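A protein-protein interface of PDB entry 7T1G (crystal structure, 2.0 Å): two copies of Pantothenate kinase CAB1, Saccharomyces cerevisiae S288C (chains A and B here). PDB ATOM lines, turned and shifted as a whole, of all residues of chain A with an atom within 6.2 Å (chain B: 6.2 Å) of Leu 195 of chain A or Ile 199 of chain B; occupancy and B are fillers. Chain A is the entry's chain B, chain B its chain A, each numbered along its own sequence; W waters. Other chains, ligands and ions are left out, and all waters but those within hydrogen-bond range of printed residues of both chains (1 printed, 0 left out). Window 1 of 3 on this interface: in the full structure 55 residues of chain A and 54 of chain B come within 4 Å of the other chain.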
ATOM      1  N   GLY A 190      28.091  -0.905 -30.330  1.00  0.00           N
ATOM      2  CA  GLY A 190      27.935  -0.563 -28.921  1.00  0.00           C
ATOM      3  C   GLY A 190      26.490  -0.242 -28.558  1.00  0.00           C
ATOM      4  O   GLY A 190      26.061  -0.449 -27.416  1.00  0.00           O
ATOM      5  N   THR A 191      25.740   0.304 -29.519  1.00  0.00           N
ATOM      6  CA  THR A 191      24.347   0.628 -29.255  1.00  0.00           C
ATOM      7  C   THR A 191      23.561  -0.672 -29.130  1.00  0.00           C
ATOM      8  O   THR A 191      22.705  -0.817 -28.245  1.00  0.00           O
ATOM      9  CB  THR A 191      23.732   1.434 -30.415  1.00  0.00           C
ATOM     10  OG1 THR A 191      24.575   2.531 -30.780  1.00  0.00           O
ATOM     11  CG2 THR A 191      22.334   1.950 -30.124  1.00  0.00           C
ATOM     12  N   LEU A 192      23.810  -1.596 -30.068  1.00  0.00           N
ATOM     13  CA  LEU A 192      23.167  -2.901 -29.999  1.00  0.00           C
ATOM     14  C   LEU A 192      23.491  -3.603 -28.679  1.00  0.00           C
ATOM     15  O   LEU A 192      22.577  -4.080 -28.003  1.00  0.00           O
ATOM     16  CB  LEU A 192      23.606  -3.785 -31.173  1.00  0.00           C
ATOM     17  CG  LEU A 192      22.850  -5.118 -31.248  1.00  0.00           C
ATOM     18  CD1 LEU A 192      21.349  -4.858 -31.445  1.00  0.00           C
ATOM     19  CD2 LEU A 192      23.368  -5.970 -32.404  1.00  0.00           C
ATOM     20  N   TRP A 193      24.791  -3.713 -28.368  1.00  0.00           N
ATOM     21  CA  TRP A 193      25.272  -4.434 -27.189  1.00  0.00           C
ATOM     22  C   TRP A 193      24.762  -3.754 -25.920  1.00  0.00           C
ATOM     23  O   TRP A 193      24.250  -4.413 -25.041  1.00  0.00           O
ATOM     24  CB  TRP A 193      26.818  -4.593 -27.190  1.00  0.00           C
ATOM     25  CG  TRP A 193      27.402  -5.066 -28.495  1.00  0.00           C
ATOM     26  CD1 TRP A 193      26.855  -6.004 -29.325  1.00  0.00           C
ATOM     27  CD2 TRP A 193      28.639  -4.650 -29.125  1.00  0.00           C
ATOM     28  NE1 TRP A 193      27.667  -6.205 -30.413  1.00  0.00           N
ATOM     29  CE2 TRP A 193      28.762  -5.384 -30.330  1.00  0.00           C
ATOM     30  CE3 TRP A 193      29.637  -3.697 -28.835  1.00  0.00           C
ATOM     31  CZ2 TRP A 193      29.809  -5.172 -31.244  1.00  0.00           C
ATOM     32  CZ3 TRP A 193      30.703  -3.530 -29.707  1.00  0.00           C
ATOM     33  CH2 TRP A 193      30.792  -4.264 -30.902  1.00  0.00           C
ATOM     34  N   GLY A 194      24.844  -2.425 -25.868  1.00  0.00           N
ATOM     35  CA  GLY A 194      24.365  -1.618 -24.759  1.00  0.00           C
ATOM     36  C   GLY A 194      22.878  -1.844 -24.493  1.00  0.00           C
ATOM     37  O   GLY A 194      22.509  -2.193 -23.381  1.00  0.00           O
ATOM     38  N   LEU A 195      22.038  -1.685 -25.521  1.00  0.00           N
ATOM     39  CA  LEU A 195      20.601  -1.813 -25.357  1.00  0.00           C
ATOM     40  C   LEU A 195      20.291  -3.222 -24.876  1.00  0.00           C
ATOM     41  O   LEU A 195      19.466  -3.379 -24.012  1.00  0.00           O
ATOM     42  CB  LEU A 195      19.853  -1.476 -26.657  1.00  0.00           C
ATOM     43  CG  LEU A 195      19.776   0.020 -26.984  1.00  0.00           C
ATOM     44  CD1 LEU A 195      19.174   0.228 -28.374  1.00  0.00           C
ATOM     45  CD2 LEU A 195      18.937   0.761 -25.929  1.00  0.00           C
ATOM     46  N   LEU A 196      20.929  -4.240 -25.463  1.00  0.00           N
ATOM     47  CA  LEU A 196      20.482  -5.607 -25.210  1.00  0.00           C
ATOM     48  C   LEU A 196      20.983  -6.104 -23.842  1.00  0.00           C
ATOM     49  O   LEU A 196      20.321  -6.903 -23.173  1.00  0.00           O
ATOM     50  CB  LEU A 196      20.963  -6.515 -26.345  1.00  0.00           C
ATOM     51  CG  LEU A 196      20.234  -6.395 -27.698  1.00  0.00           C
ATOM     52  CD1 LEU A 196      20.656  -7.568 -28.592  1.00  0.00           C
ATOM     53  CD2 LEU A 196      18.726  -6.416 -27.516  1.00  0.00           C
ATOM     54  N   SER A 197      22.179  -5.663 -23.447  1.00  0.00           N
ATOM     55  CA  SER A 197      22.682  -5.890 -22.100  1.00  0.00           C
ATOM     56  C   SER A 197      21.675  -5.405 -21.061  1.00  0.00           C
ATOM     57  O   SER A 197      21.252  -6.181 -20.202  1.00  0.00           O
ATOM     58  CB  SER A 197      23.996  -5.177 -21.894  1.00  0.00           C
ATOM     59  OG  SER A 197      24.988  -5.863 -22.607  1.00  0.00           O
ATOM     60  N   LEU A 198      21.372  -4.098 -21.105  1.00  0.00           N
ATOM     61  CA  LEU A 198      20.518  -3.450 -20.118  1.00  0.00           C
ATOM     62  C   LEU A 198      19.131  -4.085 -20.125  1.00  0.00           C
ATOM     63  O   LEU A 198      18.541  -4.302 -19.078  1.00  0.00           O
ATOM     64  CB  LEU A 198      20.412  -1.956 -20.450  1.00  0.00           C
ATOM     65  CG  LEU A 198      19.790  -1.085 -19.352  1.00  0.00           C
ATOM     66  CD1 LEU A 198      20.411  -1.407 -17.989  1.00  0.00           C
ATOM     67  CD2 LEU A 198      19.931   0.393 -19.655  1.00  0.00           C
ATOM     68  N   ILE A 199      18.565  -4.296 -21.322  1.00  0.00           N
ATOM     69  CA  ILE A 199      17.176  -4.721 -21.397  1.00  0.00           C
ATOM     70  C   ILE A 199      17.063  -6.195 -21.019  1.00  0.00           C
ATOM     71  O   ILE A 199      16.154  -6.559 -20.294  1.00  0.00           O
ATOM     72  CB  ILE A 199      16.567  -4.466 -22.788  1.00  0.00           C
ATOM     73  CG1 ILE A 199      16.378  -2.962 -23.034  1.00  0.00           C
ATOM     74  CG2 ILE A 199      15.242  -5.213 -22.903  1.00  0.00           C
ATOM     75  CD1 ILE A 199      16.184  -2.613 -24.501  1.00  0.00           C
ATOM     76  N   THR A 200      17.937  -7.054 -21.559  1.00  0.00           N
ATOM     77  CA  THR A 200      17.700  -8.485 -21.425  1.00  0.00           C
ATOM     78  C   THR A 200      18.650  -9.149 -20.425  1.00  0.00           C
ATOM     79  O   THR A 200      18.396 -10.277 -20.021  1.00  0.00           O
ATOM     80  CB  THR A 200      17.928  -9.231 -22.743  1.00  0.00           C
ATOM     81  OG1 THR A 200      19.332  -9.300 -22.975  1.00  0.00           O
ATOM     82  CG2 THR A 200      17.232  -8.606 -23.937  1.00  0.00           C
ATOM     83  N   ILE A 287      13.174  -9.480 -28.530  1.00  0.00           N
ATOM     84  CA  ILE A 287      13.826  -8.196 -28.338  1.00  0.00           C
ATOM     85  C   ILE A 287      15.180  -8.217 -29.051  1.00  0.00           C
ATOM     86  O   ILE A 287      15.545  -7.262 -29.729  1.00  0.00           O
ATOM     87  CB  ILE A 287      13.972  -7.881 -26.827  1.00  0.00           C
ATOM     88  CG1 ILE A 287      12.617  -7.568 -26.186  1.00  0.00           C
ATOM     89  CG2 ILE A 287      15.006  -6.777 -26.571  1.00  0.00           C
ATOM     90  CD1 ILE A 287      12.609  -7.670 -24.676  1.00  0.00           C
ATOM     91  N   LEU A 291      16.106  -5.690 -32.276  1.00  0.00           N
ATOM     92  CA  LEU A 291      17.117  -4.650 -32.195  1.00  0.00           C
ATOM     93  C   LEU A 291      18.279  -4.962 -33.126  1.00  0.00           C
ATOM     94  O   LEU A 291      18.915  -4.041 -33.632  1.00  0.00           O
ATOM     95  CB  LEU A 291      17.556  -4.492 -30.729  1.00  0.00           C
ATOM     96  CG  LEU A 291      16.497  -3.788 -29.864  1.00  0.00           C
ATOM     97  CD1 LEU A 291      17.100  -3.249 -28.585  1.00  0.00           C
ATOM     98  CD2 LEU A 291      15.797  -2.665 -30.645  1.00  0.00           C
ATOM     99  N   ILE A 295      19.191  -2.107 -35.907  1.00  0.00           N
ATOM    100  CA  ILE A 295      20.528  -1.533 -35.986  1.00  0.00           C
ATOM    101  C   ILE A 295      21.134  -1.949 -37.335  1.00  0.00           C
ATOM    102  O   ILE A 295      21.747  -1.146 -38.032  1.00  0.00           O
ATOM    103  CB  ILE A 295      21.407  -1.931 -34.769  1.00  0.00           C
ATOM    104  CG1 ILE A 295      20.903  -1.359 -33.437  1.00  0.00           C
ATOM    105  CG2 ILE A 295      22.882  -1.568 -34.979  1.00  0.00           C
ATOM    106  CD1 ILE A 295      20.792   0.147 -33.350  1.00  0.00           C
ATOM    107  N   GLY B 194       9.017   3.180 -27.409  1.00  0.00           N
ATOM    108  CA  GLY B 194       9.113   1.787 -26.982  1.00  0.00           C
ATOM    109  C   GLY B 194      10.286   1.534 -26.023  1.00  0.00           C
ATOM    110  O   GLY B 194      10.123   0.960 -24.963  1.00  0.00           O
ATOM    111  N   LEU B 195      11.484   1.962 -26.417  1.00  0.00           N
ATOM    112  CA  LEU B 195      12.713   1.696 -25.706  1.00  0.00           C
ATOM    113  C   LEU B 195      12.654   2.405 -24.361  1.00  0.00           C
ATOM    114  O   LEU B 195      12.995   1.801 -23.355  1.00  0.00           O
ATOM    115  CB  LEU B 195      13.876   2.254 -26.545  1.00  0.00           C
ATOM    116  CG  LEU B 195      14.307   1.393 -27.746  1.00  0.00           C
ATOM    117  CD1 LEU B 195      15.431   2.070 -28.520  1.00  0.00           C
ATOM    118  CD2 LEU B 195      14.770   0.010 -27.278  1.00  0.00           C
ATOM    119  N   LEU B 196      12.258   3.691 -24.339  1.00  0.00           N
ATOM    120  CA  LEU B 196      12.356   4.433 -23.085  1.00  0.00           C
ATOM    121  C   LEU B 196      11.240   4.022 -22.123  1.00  0.00           C
ATOM    122  O   LEU B 196      11.431   3.983 -20.910  1.00  0.00           O
ATOM    123  CB  LEU B 196      12.332   5.944 -23.360  1.00  0.00           C
ATOM    124  CG  LEU B 196      13.610   6.479 -23.996  1.00  0.00           C
ATOM    125  CD1 LEU B 196      13.479   7.977 -24.193  1.00  0.00           C
ATOM    126  CD2 LEU B 196      14.829   6.174 -23.119  1.00  0.00           C
ATOM    127  N   SER B 197      10.072   3.722 -22.675  1.00  0.00           N
ATOM    128  CA  SER B 197       8.994   3.142 -21.884  1.00  0.00           C
ATOM    129  C   SER B 197       9.480   1.910 -21.106  1.00  0.00           C
ATOM    130  O   SER B 197       9.390   1.872 -19.877  1.00  0.00           O
ATOM    131  CB  SER B 197       7.801   2.856 -22.758  1.00  0.00           C
ATOM    132  OG  SER B 197       6.859   2.092 -22.055  1.00  0.00           O
ATOM    133  N   LEU B 198      10.056   0.934 -21.818  1.00  0.00           N
ATOM    134  CA  LEU B 198      10.499  -0.307 -21.221  1.00  0.00           C
ATOM    135  C   LEU B 198      11.698  -0.075 -20.291  1.00  0.00           C
ATOM    136  O   LEU B 198      11.745  -0.618 -19.188  1.00  0.00           O
ATOM    137  CB  LEU B 198      10.810  -1.298 -22.342  1.00  0.00           C
ATOM    138  CG  LEU B 198      11.361  -2.652 -21.887  1.00  0.00           C
ATOM    139  CD1 LEU B 198      10.358  -3.447 -21.069  1.00  0.00           C
ATOM    140  CD2 LEU B 198      11.843  -3.497 -23.050  1.00  0.00           C
ATOM    141  N   ILE B 199      12.658   0.757 -20.712  1.00  0.00           N
ATOM    142  CA  ILE B 199      13.883   0.898 -19.941  1.00  0.00           C
ATOM    143  C   ILE B 199      13.663   1.779 -18.708  1.00  0.00           C
ATOM    144  O   ILE B 199      14.181   1.463 -17.627  1.00  0.00           O
ATOM    145  CB  ILE B 199      15.062   1.399 -20.808  1.00  0.00           C
ATOM    146  CG1 ILE B 199      15.378   0.403 -21.932  1.00  0.00           C
ATOM    147  CG2 ILE B 199      16.296   1.694 -19.937  1.00  0.00           C
ATOM    148  CD1 ILE B 199      16.479   0.878 -22.866  1.00  0.00           C
ATOM    149  N   THR B 200      12.961   2.905 -18.867  1.00  0.00           N
ATOM    150  CA  THR B 200      12.964   3.905 -17.802  1.00  0.00           C
ATOM    151  C   THR B 200      11.669   3.885 -16.993  1.00  0.00           C
ATOM    152  O   THR B 200      11.596   4.538 -15.944  1.00  0.00           O
ATOM    153  CB  THR B 200      13.257   5.325 -18.306  1.00  0.00           C
ATOM    154  OG1 THR B 200      12.071   5.770 -18.953  1.00  0.00           O
ATOM    155  CG2 THR B 200      14.444   5.419 -19.239  1.00  0.00           C
ATOM    156  N   GLY B 201      10.640   3.187 -17.493  1.00  0.00           N
ATOM    157  CA  GLY B 201       9.342   3.230 -16.839  1.00  0.00           C
ATOM    158  C   GLY B 201       8.543   4.497 -17.160  1.00  0.00           C
ATOM    159  O   GLY B 201       7.381   4.623 -16.749  1.00  0.00           O
ATOM    160  N   ALA B 202       9.117   5.424 -17.937  1.00  0.00           N
ATOM    161  CA  ALA B 202       8.436   6.689 -18.193  1.00  0.00           C
ATOM    162  C   ALA B 202       7.013   6.421 -18.707  1.00  0.00           C
ATOM    163  O   ALA B 202       6.794   5.537 -19.519  1.00  0.00           O
ATOM    164  CB  ALA B 202       9.248   7.518 -19.157  1.00  0.00           C
ATOM    165  N   PHE B 246      24.779   4.861 -26.324  1.00  0.00           N
ATOM    166  CA  PHE B 246      24.670   3.727 -25.400  1.00  0.00           C
ATOM    167  C   PHE B 246      25.931   2.868 -25.359  1.00  0.00           C
ATOM    168  O   PHE B 246      25.930   1.756 -24.801  1.00  0.00           O
ATOM    169  CB  PHE B 246      23.472   2.831 -25.753  1.00  0.00           C
ATOM    170  CG  PHE B 246      22.417   2.788 -24.667  1.00  0.00           C
ATOM    171  CD1 PHE B 246      21.781   3.946 -24.251  1.00  0.00           C
ATOM    172  CD2 PHE B 246      22.088   1.590 -24.040  1.00  0.00           C
ATOM    173  CE1 PHE B 246      20.834   3.926 -23.233  1.00  0.00           C
ATOM    174  CE2 PHE B 246      21.142   1.559 -23.019  1.00  0.00           C
ATOM    175  CZ  PHE B 246      20.520   2.724 -22.610  1.00  0.00           C
ATOM    176  N   VAL B 249      27.370   1.343 -22.066  1.00  0.00           N
ATOM    177  CA  VAL B 249      26.475   0.580 -21.211  1.00  0.00           C
ATOM    178  C   VAL B 249      26.928  -0.870 -21.103  1.00  0.00           C
ATOM    179  O   VAL B 249      26.872  -1.427 -20.021  1.00  0.00           O
ATOM    180  CB  VAL B 249      24.990   0.705 -21.613  1.00  0.00           C
ATOM    181  CG1 VAL B 249      24.112  -0.312 -20.899  1.00  0.00           C
ATOM    182  CG2 VAL B 249      24.478   2.113 -21.373  1.00  0.00           C
ATOM    183  N   HIS B 271      10.085  -3.699 -17.406  1.00  0.00           N
ATOM    184  CA  HIS B 271      10.684  -2.598 -16.677  1.00  0.00           C
ATOM    185  C   HIS B 271      11.165  -3.116 -15.315  1.00  0.00           C
ATOM    186  O   HIS B 271      12.304  -2.867 -14.878  1.00  0.00           O
ATOM    187  CB  HIS B 271       9.719  -1.398 -16.580  1.00  0.00           C
ATOM    188  CG  HIS B 271      10.297  -0.292 -15.761  1.00  0.00           C
ATOM    189  ND1 HIS B 271      11.554   0.224 -16.015  1.00  0.00           N
ATOM    190  CD2 HIS B 271       9.850   0.335 -14.645  1.00  0.00           C
ATOM    191  CE1 HIS B 271      11.849   1.153 -15.121  1.00  0.00           C
ATOM    192  NE2 HIS B 271      10.817   1.227 -14.263  1.00  0.00           N
ATOM    193  N   ILE B 274      14.312  -5.047 -15.383  1.00  0.00           N
ATOM    194  CA  ILE B 274      15.414  -4.207 -15.812  1.00  0.00           C
ATOM    195  C   ILE B 274      15.886  -3.409 -14.596  1.00  0.00           C
ATOM    196  O   ILE B 274      17.056  -3.053 -14.492  1.00  0.00           O
ATOM    197  CB  ILE B 274      14.986  -3.340 -17.013  1.00  0.00           C
ATOM    198  CG1 ILE B 274      14.857  -4.204 -18.286  1.00  0.00           C
ATOM    199  CG2 ILE B 274      15.957  -2.182 -17.215  1.00  0.00           C
ATOM    200  CD1 ILE B 274      14.157  -3.527 -19.460  1.00  0.00           C
ATOM    201  N   GLU B 275      14.956  -3.153 -13.667  1.00  0.00           N
ATOM    202  CA  GLU B 275      15.251  -2.317 -12.518  1.00  0.00           C
ATOM    203  C   GLU B 275      15.879  -3.151 -11.419  1.00  0.00           C
ATOM    204  O   GLU B 275      16.826  -2.690 -10.810  1.00  0.00           O
ATOM    205  CB  GLU B 275      14.001  -1.601 -12.019  1.00  0.00           C
ATOM    206  CG  GLU B 275      14.047  -0.130 -12.337  1.00  0.00           C
ATOM    207  CD  GLU B 275      13.280   0.730 -11.350  1.00  0.00           C
ATOM    208  OE1 GLU B 275      12.731   0.172 -10.353  1.00  0.00           O
ATOM    209  OE2 GLU B 275      13.217   1.962 -11.592  1.00  0.00           O
ATOM    210  N   ASN B 284      17.830   7.547 -15.380  1.00  0.00           N
ATOM    211  CA  ASN B 284      16.719   7.661 -16.296  1.00  0.00           C
ATOM    212  C   ASN B 284      16.924   8.890 -17.177  1.00  0.00           C
ATOM    213  O   ASN B 284      16.849   8.757 -18.405  1.00  0.00           O
ATOM    214  CB  ASN B 284      15.363   7.546 -15.566  1.00  0.00           C
ATOM    215  CG  ASN B 284      15.002   6.105 -15.267  1.00  0.00           C
ATOM    216  OD1 ASN B 284      15.648   5.178 -15.756  1.00  0.00           O
ATOM    217  ND2 ASN B 284      13.983   5.905 -14.459  1.00  0.00           N
ATOM    218  N   ILE B 287      19.592   8.188 -19.844  1.00  0.00           N
ATOM    219  CA  ILE B 287      19.105   7.233 -20.832  1.00  0.00           C
ATOM    220  C   ILE B 287      18.179   7.947 -21.823  1.00  0.00           C
ATOM    221  O   ILE B 287      18.243   7.683 -23.023  1.00  0.00           O
ATOM    222  CB  ILE B 287      18.427   6.019 -20.152  1.00  0.00           C
ATOM    223  CG1 ILE B 287      19.433   5.240 -19.300  1.00  0.00           C
ATOM    224  CG2 ILE B 287      17.745   5.114 -21.185  1.00  0.00           C
ATOM    225  CD1 ILE B 287      18.796   4.171 -18.425  1.00  0.00           C
ATOM    226  N   LEU B 291      18.972   8.539 -25.891  1.00  0.00           N
ATOM    227  CA  LEU B 291      18.231   7.883 -26.956  1.00  0.00           C
ATOM    228  C   LEU B 291      17.455   8.913 -27.764  1.00  0.00           C
ATOM    229  O   LEU B 291      17.210   8.696 -28.941  1.00  0.00           O
ATOM    230  CB  LEU B 291      17.262   6.849 -26.375  1.00  0.00           C
ATOM    231  CG  LEU B 291      17.936   5.602 -25.822  1.00  0.00           C
ATOM    232  CD1 LEU B 291      16.937   4.467 -25.747  1.00  0.00           C
ATOM    233  CD2 LEU B 291      19.141   5.178 -26.641  1.00  0.00           C
HETATM  234  O   HOH W   1      27.591  -1.039 -24.819  1.00  0.00           O
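Among the printed residues, pairs that only touch across the chains: Ile 199 of chain A with Ile 274 of chain B, Gly 194 of chain A with Val 249 of chain B, Gly 194 of chain A with Phe 246 of chain B, Leu 195 of chain A with Phe 246 of chain B, Ile 199 of chain A with Ile 199 of chain B, Leu 198 of chain A with Phe 246 of chain B, Leu 198 of chain A with Ile 274 of chain B, Ile 199 of chain A with Leu 198 of chain B, Leu 198 of chain A with Ile 199 of chain B and Leu 195 of chain A with Ile 199 of chain B.
Hydrophobic or aromatic side chains of chain A within 4 Å of the printed part of chain B: Leu 195, Leu 198 and Ile 199. Of the 17 printed residues of chain B, 5 touch a printed residue of chain A. Hydrophobic or aromatic side chains of chain B that line the printed part of chain A: Leu 198, Ile 199, Phe 246, Val 249 and Ile 274. Among the printed residues, no Asp or Glu carboxylate lies within 4 Å of a Lys or Arg side-chain nitrogen of the other chain.
Water W1 lies within hydrogen-bond range of the backbone carbonyl oxygen of Gly 190 of chain A (3.1 Å), the backbone NH of Gly 194 of chain A (3.3 Å) and the backbone carbonyl oxygen of Phe 246 of chain B (3.3 Å).
Leu 195 of chain A touches Ile 199 of chain B, but with the chains exchanged Ile 199 of chain A does not touch Leu 195 of chain B (4.1 Å). Leu 198 of chain A touches Ile 199 of chain B, and with the chains exchanged Ile 199 of chain A touches Leu 198 of chain B. Ile 199 of chain A touches its own counterpart, Ile 199 of chain B.
O of Leu 198 of chain B sits at hydrogen-bond distance from ND1 of His 271 of chain B (3.3 Å). The backbone carbonyl oxygen of Ile 199 of chain B is in hydrogen-bond range of a ring nitrogen (ND1) of His 271 of chain B (3.3 Å).
The backbone carbonyl oxygen of Phe 246 of chain B sits close to the backbone carbonyl oxygen of Gly 190 of chain A, at 3.4 Å.
Of chain B, only Ile 199 (3.9 Å) and Phe 246 (3.6 Å) come within 4 Å of Leu 195 of chain A. Ile 199 of chain B touches just these residues of chain A: Leu 195, Leu 198 and Ile 199. Printed residues of chain B within 4 Å of Gly 194 of chain A: Phe 246 (3.6 Å) and Val 249 (3.5 Å). Of the printed residues of chain A, Ile 274 of chain B touches Leu 198 (3.8 Å) and Ile 199 (3.4 Å). Of the printed residues of chain A, Leu 198 of chain B touches Ile 199 (3.8 Å). Of the printed residues of chain B, Ile 199 of chain A touches Leu 198, Ile 199 and Ile 274. Leu 291 of chain B touches none of the printed residues of chain A. Ser 197 of chain B touches none of the printed residues of chain A. The nearest printed residue of chain A that does not touch Ile 199 of chain B is Gly 194 of chain A (6.8 Å). The nearest printed residue of chain A that does not touch Leu 198 of chain B is Ile 287 of chain A (4.5 Å).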
